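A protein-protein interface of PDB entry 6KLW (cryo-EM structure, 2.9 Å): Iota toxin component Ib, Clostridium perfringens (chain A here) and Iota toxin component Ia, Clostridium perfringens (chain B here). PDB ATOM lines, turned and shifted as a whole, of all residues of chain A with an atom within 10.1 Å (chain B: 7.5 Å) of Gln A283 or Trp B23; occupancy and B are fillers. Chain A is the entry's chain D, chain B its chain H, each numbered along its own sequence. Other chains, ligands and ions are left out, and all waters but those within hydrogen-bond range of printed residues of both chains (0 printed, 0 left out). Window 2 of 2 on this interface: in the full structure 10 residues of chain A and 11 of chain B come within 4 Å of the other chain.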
ATOM      1  N   THR A 279      -6.036 -31.325   9.148  1.00  0.00           N
ATOM      2  CA  THR A 279      -5.044 -31.930   8.274  1.00  0.00           C
ATOM      3  C   THR A 279      -3.679 -31.793   8.926  1.00  0.00           C
ATOM      4  O   THR A 279      -3.477 -30.962   9.812  1.00  0.00           O
ATOM      5  CB  THR A 279      -5.021 -31.289   6.881  1.00  0.00           C
ATOM      6  OG1 THR A 279      -4.481 -29.964   6.965  1.00  0.00           O
ATOM      7  CG2 THR A 279      -6.413 -31.222   6.295  1.00  0.00           C
ATOM      8  N   LYS A 280      -2.739 -32.613   8.476  1.00  0.00           N
ATOM      9  CA  LYS A 280      -1.358 -32.544   8.932  1.00  0.00           C
ATOM     10  C   LYS A 280      -0.583 -31.610   8.012  1.00  0.00           C
ATOM     11  O   LYS A 280      -0.584 -31.794   6.791  1.00  0.00           O
ATOM     12  CB  LYS A 280      -0.721 -33.933   8.956  1.00  0.00           C
ATOM     13  CG  LYS A 280      -1.001 -34.708  10.224  1.00  0.00           C
ATOM     14  CD  LYS A 280      -1.121 -36.195   9.941  1.00  0.00           C
ATOM     15  CE  LYS A 280      -1.771 -36.932  11.102  1.00  0.00           C
ATOM     16  NZ  LYS A 280      -3.119 -36.396  11.412  1.00  0.00           N
ATOM     17  N   ASN A 281       0.079 -30.614   8.598  1.00  0.00           N
ATOM     18  CA  ASN A 281       0.845 -29.652   7.815  1.00  0.00           C
ATOM     19  C   ASN A 281       2.181 -30.264   7.413  1.00  0.00           C
ATOM     20  O   ASN A 281       2.332 -31.488   7.444  1.00  0.00           O
ATOM     21  CB  ASN A 281       1.036 -28.338   8.581  1.00  0.00           C
ATOM     22  CG  ASN A 281       1.867 -28.501   9.830  1.00  0.00           C
ATOM     23  OD1 ASN A 281       2.015 -29.599  10.352  1.00  0.00           O
ATOM     24  ND2 ASN A 281       2.412 -27.399  10.322  1.00  0.00           N
ATOM     25  N   SER A 282       3.134 -29.430   6.986  1.00  0.00           N
ATOM     26  CA  SER A 282       4.408 -29.935   6.479  1.00  0.00           C
ATOM     27  C   SER A 282       5.082 -30.893   7.455  1.00  0.00           C
ATOM     28  O   SER A 282       5.756 -31.837   7.030  1.00  0.00           O
ATOM     29  CB  SER A 282       5.343 -28.772   6.155  1.00  0.00           C
ATOM     30  OG  SER A 282       6.580 -29.242   5.648  1.00  0.00           O
ATOM     31  N   GLN A 283       4.921 -30.671   8.757  1.00  0.00           N
ATOM     32  CA  GLN A 283       5.370 -31.606   9.777  1.00  0.00           C
ATOM     33  C   GLN A 283       4.161 -32.332  10.365  1.00  0.00           C
ATOM     34  O   GLN A 283       3.028 -32.181   9.898  1.00  0.00           O
ATOM     35  CB  GLN A 283       6.190 -30.885  10.849  1.00  0.00           C
ATOM     36  CG  GLN A 283       5.499 -29.706  11.500  1.00  0.00           C
ATOM     37  CD  GLN A 283       5.768 -28.406  10.775  1.00  0.00           C
ATOM     38  OE1 GLN A 283       6.226 -28.405   9.634  1.00  0.00           O
ATOM     39  NE2 GLN A 283       5.492 -27.289  11.436  1.00  0.00           N
ATOM     40  N   GLY A 284       4.400 -33.129  11.396  1.00  0.00           N
ATOM     41  CA  GLY A 284       3.349 -33.957  11.955  1.00  0.00           C
ATOM     42  C   GLY A 284       2.310 -33.215  12.768  1.00  0.00           C
ATOM     43  O   GLY A 284       1.593 -33.827  13.564  1.00  0.00           O
ATOM     44  N   GLN A 285       2.214 -31.903  12.583  1.00  0.00           N
ATOM     45  CA  GLN A 285       1.271 -31.106  13.350  1.00  0.00           C
ATOM     46  C   GLN A 285      -0.076 -31.021  12.640  1.00  0.00           C
ATOM     47  O   GLN A 285      -0.150 -30.870  11.421  1.00  0.00           O
ATOM     48  CB  GLN A 285       1.831 -29.705  13.574  1.00  0.00           C
ATOM     49  CG  GLN A 285       3.166 -29.702  14.296  1.00  0.00           C
ATOM     50  CD  GLN A 285       3.029 -29.945  15.781  1.00  0.00           C
ATOM     51  OE1 GLN A 285       1.995 -29.656  16.377  1.00  0.00           O
ATOM     52  NE2 GLN A 285       4.079 -30.475  16.391  1.00  0.00           N
ATOM     53  N   ILE A 286      -1.147 -31.125  13.421  1.00  0.00           N
ATOM     54  CA  ILE A 286      -2.510 -31.045  12.909  1.00  0.00           C
ATOM     55  C   ILE A 286      -2.935 -29.586  12.890  1.00  0.00           C
ATOM     56  O   ILE A 286      -2.728 -28.858  13.867  1.00  0.00           O
ATOM     57  CB  ILE A 286      -3.476 -31.887  13.759  1.00  0.00           C
ATOM     58  CG1 ILE A 286      -3.127 -33.367  13.657  1.00  0.00           C
ATOM     59  CG2 ILE A 286      -4.899 -31.670  13.320  1.00  0.00           C
ATOM     60  CD1 ILE A 286      -3.905 -34.226  14.606  1.00  0.00           C
ATOM     61  N   ILE A 287      -3.526 -29.157  11.781  1.00  0.00           N
ATOM     62  CA  ILE A 287      -4.019 -27.797  11.614  1.00  0.00           C
ATOM     63  C   ILE A 287      -5.506 -27.859  11.308  1.00  0.00           C
ATOM     64  O   ILE A 287      -5.948 -28.709  10.531  1.00  0.00           O
ATOM     65  CB  ILE A 287      -3.262 -27.058  10.492  1.00  0.00           C
ATOM     66  CG1 ILE A 287      -1.758 -27.133  10.728  1.00  0.00           C
ATOM     67  CG2 ILE A 287      -3.699 -25.615  10.415  1.00  0.00           C
ATOM     68  CD1 ILE A 287      -1.323 -26.532  12.037  1.00  0.00           C
ATOM     69  N   GLU A 289      -7.240 -24.544  11.107  1.00  0.00           N
ATOM     70  CA  GLU A 289      -7.558 -23.119  11.092  1.00  0.00           C
ATOM     71  C   GLU A 289      -8.223 -22.671   9.794  1.00  0.00           C
ATOM     72  O   GLU A 289      -9.330 -22.127   9.819  1.00  0.00           O
ATOM     73  CB  GLU A 289      -6.295 -22.293  11.351  1.00  0.00           C
ATOM     74  CG  GLU A 289      -5.733 -22.484  12.746  1.00  0.00           C
ATOM     75  CD  GLU A 289      -6.675 -21.991  13.835  1.00  0.00           C
ATOM     76  OE1 GLU A 289      -7.406 -21.006  13.600  1.00  0.00           O
ATOM     77  OE2 GLU A 289      -6.683 -22.597  14.930  1.00  0.00           O
ATOM     78  N   GLN B  22       1.685 -19.577   5.800  1.00  0.00           N
ATOM     79  CA  GLN B  22       1.414 -19.390   7.218  1.00  0.00           C
ATOM     80  C   GLN B  22       2.576 -19.868   8.100  1.00  0.00           C
ATOM     81  O   GLN B  22       3.230 -19.054   8.753  1.00  0.00           O
ATOM     82  CB  GLN B  22       0.087 -20.076   7.593  1.00  0.00           C
ATOM     83  CG  GLN B  22       0.015 -21.583   7.350  1.00  0.00           C
ATOM     84  CD  GLN B  22      -1.107 -22.248   8.118  1.00  0.00           C
ATOM     85  OE1 GLN B  22      -2.137 -21.634   8.391  1.00  0.00           O
ATOM     86  NE2 GLN B  22      -0.911 -23.511   8.475  1.00  0.00           N
ATOM     87  N   TRP B  23       2.843 -21.175   8.117  1.00  0.00           N
ATOM     88  CA  TRP B  23       3.973 -21.690   8.883  1.00  0.00           C
ATOM     89  C   TRP B  23       5.287 -21.401   8.170  1.00  0.00           C
ATOM     90  O   TRP B  23       6.215 -20.837   8.764  1.00  0.00           O
ATOM     91  CB  TRP B  23       3.812 -23.193   9.122  1.00  0.00           C
ATOM     92  CG  TRP B  23       5.105 -23.883   9.470  1.00  0.00           C
ATOM     93  CD1 TRP B  23       5.696 -23.945  10.700  1.00  0.00           C
ATOM     94  CD2 TRP B  23       5.964 -24.610   8.578  1.00  0.00           C
ATOM     95  NE1 TRP B  23       6.868 -24.658  10.627  1.00  0.00           N
ATOM     96  CE2 TRP B  23       7.055 -25.078   9.337  1.00  0.00           C
ATOM     97  CE3 TRP B  23       5.916 -24.908   7.212  1.00  0.00           C
ATOM     98  CZ2 TRP B  23       8.088 -25.829   8.775  1.00  0.00           C
ATOM     99  CZ3 TRP B  23       6.944 -25.653   6.657  1.00  0.00           C
ATOM    100  CH2 TRP B  23       8.014 -26.104   7.438  1.00  0.00           C
ATOM    101  N   GLU B  24       5.376 -21.779   6.891  1.00  0.00           N
ATOM    102  CA  GLU B  24       6.608 -21.565   6.144  1.00  0.00           C
ATOM    103  C   GLU B  24       6.886 -20.083   5.941  1.00  0.00           C
ATOM    104  O   GLU B  24       8.042 -19.666   6.015  1.00  0.00           O
ATOM    105  CB  GLU B  24       6.545 -22.299   4.801  1.00  0.00           C
ATOM    106  CG  GLU B  24       5.602 -21.691   3.768  1.00  0.00           C
ATOM    107  CD  GLU B  24       4.146 -22.063   3.994  1.00  0.00           C
ATOM    108  OE1 GLU B  24       3.805 -22.538   5.097  1.00  0.00           O
ATOM    109  OE2 GLU B  24       3.339 -21.878   3.060  1.00  0.00           O
ATOM    110  N   LYS B  25       5.843 -19.274   5.730  1.00  0.00           N
ATOM    111  CA  LYS B  25       6.033 -17.831   5.631  1.00  0.00           C
ATOM    112  C   LYS B  25       6.641 -17.273   6.910  1.00  0.00           C
ATOM    113  O   LYS B  25       7.624 -16.521   6.868  1.00  0.00           O
ATOM    114  CB  LYS B  25       4.698 -17.149   5.334  1.00  0.00           C
ATOM    115  CG  LYS B  25       4.055 -17.548   4.012  1.00  0.00           C
ATOM    116  CD  LYS B  25       4.841 -17.033   2.816  1.00  0.00           C
ATOM    117  CE  LYS B  25       4.692 -15.526   2.668  1.00  0.00           C
ATOM    118  NZ  LYS B  25       5.376 -15.007   1.453  1.00  0.00           N
ATOM    119  N   LYS B  26       6.076 -17.648   8.059  1.00  0.00           N
ATOM    120  CA  LYS B  26       6.569 -17.161   9.342  1.00  0.00           C
ATOM    121  C   LYS B  26       8.014 -17.579   9.574  1.00  0.00           C
ATOM    122  O   LYS B  26       8.880 -16.741   9.859  1.00  0.00           O
ATOM    123  CB  LYS B  26       5.671 -17.686  10.464  1.00  0.00           C
ATOM    124  CG  LYS B  26       6.004 -17.176  11.855  1.00  0.00           C
ATOM    125  CD  LYS B  26       5.247 -17.974  12.910  1.00  0.00           C
ATOM    126  CE  LYS B  26       5.097 -17.193  14.205  1.00  0.00           C
ATOM    127  NZ  LYS B  26       5.077 -18.085  15.397  1.00  0.00           N
ATOM    128  N   GLU B  27       8.295 -18.878   9.451  1.00  0.00           N
ATOM    129  CA  GLU B  27       9.637 -19.367   9.748  1.00  0.00           C
ATOM    130  C   GLU B  27      10.661 -18.826   8.755  1.00  0.00           C
ATOM    131  O   GLU B  27      11.802 -18.538   9.131  1.00  0.00           O
ATOM    132  CB  GLU B  27       9.637 -20.898   9.804  1.00  0.00           C
ATOM    133  CG  GLU B  27       9.239 -21.621   8.533  1.00  0.00           C
ATOM    134  CD  GLU B  27      10.425 -22.044   7.702  1.00  0.00           C
ATOM    135  OE1 GLU B  27      11.541 -22.114   8.260  1.00  0.00           O
ATOM    136  OE2 GLU B  27      10.234 -22.328   6.500  1.00  0.00           O
ATOM    137  N   ALA B  28      10.268 -18.651   7.492  1.00  0.00           N
ATOM    138  CA  ALA B  28      11.179 -18.104   6.494  1.00  0.00           C
ATOM    139  C   ALA B  28      11.491 -16.640   6.779  1.00  0.00           C
ATOM    140  O   ALA B  28      12.659 -16.243   6.835  1.00  0.00           O
ATOM    141  CB  ALA B  28      10.580 -18.277   5.098  1.00  0.00           C
ATOM    142  N   GLU B  29      10.453 -15.815   6.959  1.00  0.00           N
ATOM    143  CA  GLU B  29      10.658 -14.418   7.325  1.00  0.00           C
ATOM    144  C   GLU B  29      11.400 -14.260   8.644  1.00  0.00           C
ATOM    145  O   GLU B  29      11.990 -13.200   8.876  1.00  0.00           O
ATOM    146  CB  GLU B  29       9.315 -13.685   7.404  1.00  0.00           C
ATOM    147  CG  GLU B  29       8.611 -13.469   6.067  1.00  0.00           C
ATOM    148  CD  GLU B  29       9.285 -12.419   5.201  1.00  0.00           C
ATOM    149  OE1 GLU B  29       9.858 -11.460   5.760  1.00  0.00           O
ATOM    150  OE2 GLU B  29       9.236 -12.550   3.960  1.00  0.00           O
ATOM    151  N   ASP B  90      15.093 -32.021  11.824  1.00  0.00           N
ATOM    152  CA  ASP B  90      15.086 -32.991  12.908  1.00  0.00           C
ATOM    153  C   ASP B  90      14.519 -34.348  12.520  1.00  0.00           C
ATOM    154  O   ASP B  90      14.759 -35.322  13.239  1.00  0.00           O
ATOM    155  CB  ASP B  90      14.286 -32.447  14.100  1.00  0.00           C
ATOM    156  CG  ASP B  90      12.968 -31.817  13.678  1.00  0.00           C
ATOM    157  OD1 ASP B  90      12.057 -31.705  14.526  1.00  0.00           O
ATOM    158  OD2 ASP B  90      12.843 -31.435  12.496  1.00  0.00           O
ATOM    159  N   LYS B  91      13.790 -34.439  11.412  1.00  0.00           N
ATOM    160  CA  LYS B  91      13.153 -35.667  10.961  1.00  0.00           C
ATOM    161  C   LYS B  91      13.131 -35.689   9.441  1.00  0.00           C
ATOM    162  O   LYS B  91      13.193 -34.631   8.805  1.00  0.00           O
ATOM    163  CB  LYS B  91      11.720 -35.790  11.502  1.00  0.00           C
ATOM    164  CG  LYS B  91      11.652 -36.058  12.988  1.00  0.00           C
ATOM    165  CD  LYS B  91      10.232 -36.212  13.467  1.00  0.00           C
ATOM    166  CE  LYS B  91      10.215 -36.463  14.959  1.00  0.00           C
ATOM    167  NZ  LYS B  91      10.789 -37.792  15.295  1.00  0.00           N
ATOM    168  N   PRO B  92      13.051 -36.876   8.835  1.00  0.00           N
ATOM    169  CA  PRO B  92      13.031 -36.956   7.370  1.00  0.00           C
ATOM    170  C   PRO B  92      11.905 -36.130   6.769  1.00  0.00           C
ATOM    171  O   PRO B  92      10.850 -35.938   7.375  1.00  0.00           O
ATOM    172  CB  PRO B  92      12.830 -38.450   7.102  1.00  0.00           C
ATOM    173  CG  PRO B  92      13.386 -39.116   8.302  1.00  0.00           C
ATOM    174  CD  PRO B  92      13.078 -38.212   9.455  1.00  0.00           C
ATOM    175  N   ILE B  93      12.148 -35.632   5.560  1.00  0.00           N
ATOM    176  CA  ILE B  93      11.212 -34.762   4.861  1.00  0.00           C
ATOM    177  C   ILE B  93      11.081 -35.252   3.427  1.00  0.00           C
ATOM    178  O   ILE B  93      12.017 -35.824   2.863  1.00  0.00           O
ATOM    179  CB  ILE B  93      11.670 -33.282   4.928  1.00  0.00           C
ATOM    180  CG1 ILE B  93      11.247 -32.654   6.260  1.00  0.00           C
ATOM    181  CG2 ILE B  93      11.133 -32.458   3.773  1.00  0.00           C
ATOM    182  CD1 ILE B  93      11.644 -31.202   6.407  1.00  0.00           C
ATOM    183  N   LEU B 145       8.264 -28.370  -0.825  1.00  0.00           N
ATOM    184  CA  LEU B 145       7.749 -29.350   0.121  1.00  0.00           C
ATOM    185  C   LEU B 145       6.406 -29.922  -0.304  1.00  0.00           C
ATOM    186  O   LEU B 145       5.823 -30.721   0.434  1.00  0.00           O
ATOM    187  CB  LEU B 145       7.640 -28.730   1.513  1.00  0.00           C
ATOM    188  CG  LEU B 145       8.934 -28.129   2.056  1.00  0.00           C
ATOM    189  CD1 LEU B 145       8.627 -27.028   3.048  1.00  0.00           C
ATOM    190  CD2 LEU B 145       9.784 -29.206   2.694  1.00  0.00           C
ATOM    191  N   TYR B 146       5.903 -29.531  -1.474  1.00  0.00           N
ATOM    192  CA  TYR B 146       4.627 -30.011  -1.988  1.00  0.00           C
ATOM    193  C   TYR B 146       4.711 -30.144  -3.500  1.00  0.00           C
ATOM    194  O   TYR B 146       5.401 -29.357  -4.152  1.00  0.00           O
ATOM    195  CB  TYR B 146       3.486 -29.063  -1.609  1.00  0.00           C
ATOM    196  CG  TYR B 146       3.271 -28.928  -0.121  1.00  0.00           C
ATOM    197  CD1 TYR B 146       2.637 -29.929   0.601  1.00  0.00           C
ATOM    198  CD2 TYR B 146       3.701 -27.800   0.563  1.00  0.00           C
ATOM    199  CE1 TYR B 146       2.438 -29.811   1.959  1.00  0.00           C
ATOM    200  CE2 TYR B 146       3.506 -27.673   1.923  1.00  0.00           C
ATOM    201  CZ  TYR B 146       2.874 -28.683   2.616  1.00  0.00           C
ATOM    202  OH  TYR B 146       2.673 -28.567   3.971  1.00  0.00           O
ATOM    203  N   PRO B 172      14.896 -21.749   4.113  1.00  0.00           N
ATOM    204  CA  PRO B 172      13.714 -21.220   3.425  1.00  0.00           C
ATOM    205  C   PRO B 172      13.851 -19.743   3.100  1.00  0.00           C
ATOM    206  O   PRO B 172      14.028 -18.919   4.002  1.00  0.00           O
ATOM    207  CB  PRO B 172      12.590 -21.476   4.432  1.00  0.00           C
ATOM    208  CG  PRO B 172      13.271 -21.396   5.763  1.00  0.00           C
ATOM    209  CD  PRO B 172      14.723 -21.773   5.575  1.00  0.00           C
ATOM    210  N   VAL B 179       7.953 -19.327  -1.348  1.00  0.00           N
ATOM    211  CA  VAL B 179       9.021 -19.861  -0.514  1.00  0.00           C
ATOM    212  C   VAL B 179       9.738 -20.965  -1.279  1.00  0.00           C
ATOM    213  O   VAL B 179       9.098 -21.815  -1.907  1.00  0.00           O
ATOM    214  CB  VAL B 179       8.483 -20.399   0.830  1.00  0.00           C
ATOM    215  CG1 VAL B 179       9.613 -20.985   1.664  1.00  0.00           C
ATOM    216  CG2 VAL B 179       7.756 -19.306   1.596  1.00  0.00           C
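OH of Tyr B146 lies within hydrogen-bond range of N of Ser A282 (3.2 Å).
NE1 of Trp B23 lies close to NE2 of Gln A283 (3.1 Å).
The backbone carbonyl oxygen (O) of Gln A285 lies close to the side-chain amide oxygen (OD1) of Asn A281.
The backbone NH (N) of Ile A287 lies within hydrogen-bond range of the backbone carbonyl oxygen (O) of Thr A279 (2.7 Å).
The side-chain amide oxygen of Asn A281 lies close to the backbone carbonyl oxygen of Gln A283 (2.8 Å).
Among the printed residues, merely in contact across the chains: Asn A281 with Tyr B146, Ser A282 with Trp B23, Ser A282 with Leu B145 and Ile A287 with Gln B22.
Gln A283 touches one residue of chain B.
Trp B23 touches just these residues of chain A: Ser A282 and Gln A283.
No residue of chain A comes within 4 Å of Glu B24.
Printed residues of chain B within 4 Å of Asn A281: Tyr B146.
Printed residues of chain B within 4 Å of Ser A282: Trp B23 (3.5 Å), Leu B145 (3.98 Å) and Tyr B146 (3.2 Å).
Printed residues of chain A within 4 Å of Leu B145: Ser A282 (3.98 Å).
Printed residues of chain A within 4 Å of Tyr B146: Asn A281 and Ser A282.
Of the printed residues of chain B, Ile A287 touches Gln B22 (3.995 Å).
The nearest printed residue of chain B that does not touch Ser A282 is Ile B93 (5.5 Å).
Of the 10 printed residues of chain A, 4 touch a printed residue of chain B.
Hydrophobic or aromatic side chains of chain A within 4 Å of the printed part of chain B: Ile A287.
Hydrophobic or aromatic side chains of chain B within 4 Å of the printed part of chain A: Trp B23, Leu B145 and Tyr B146.
Among the printed residues, 6 pairs touch across the chains.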
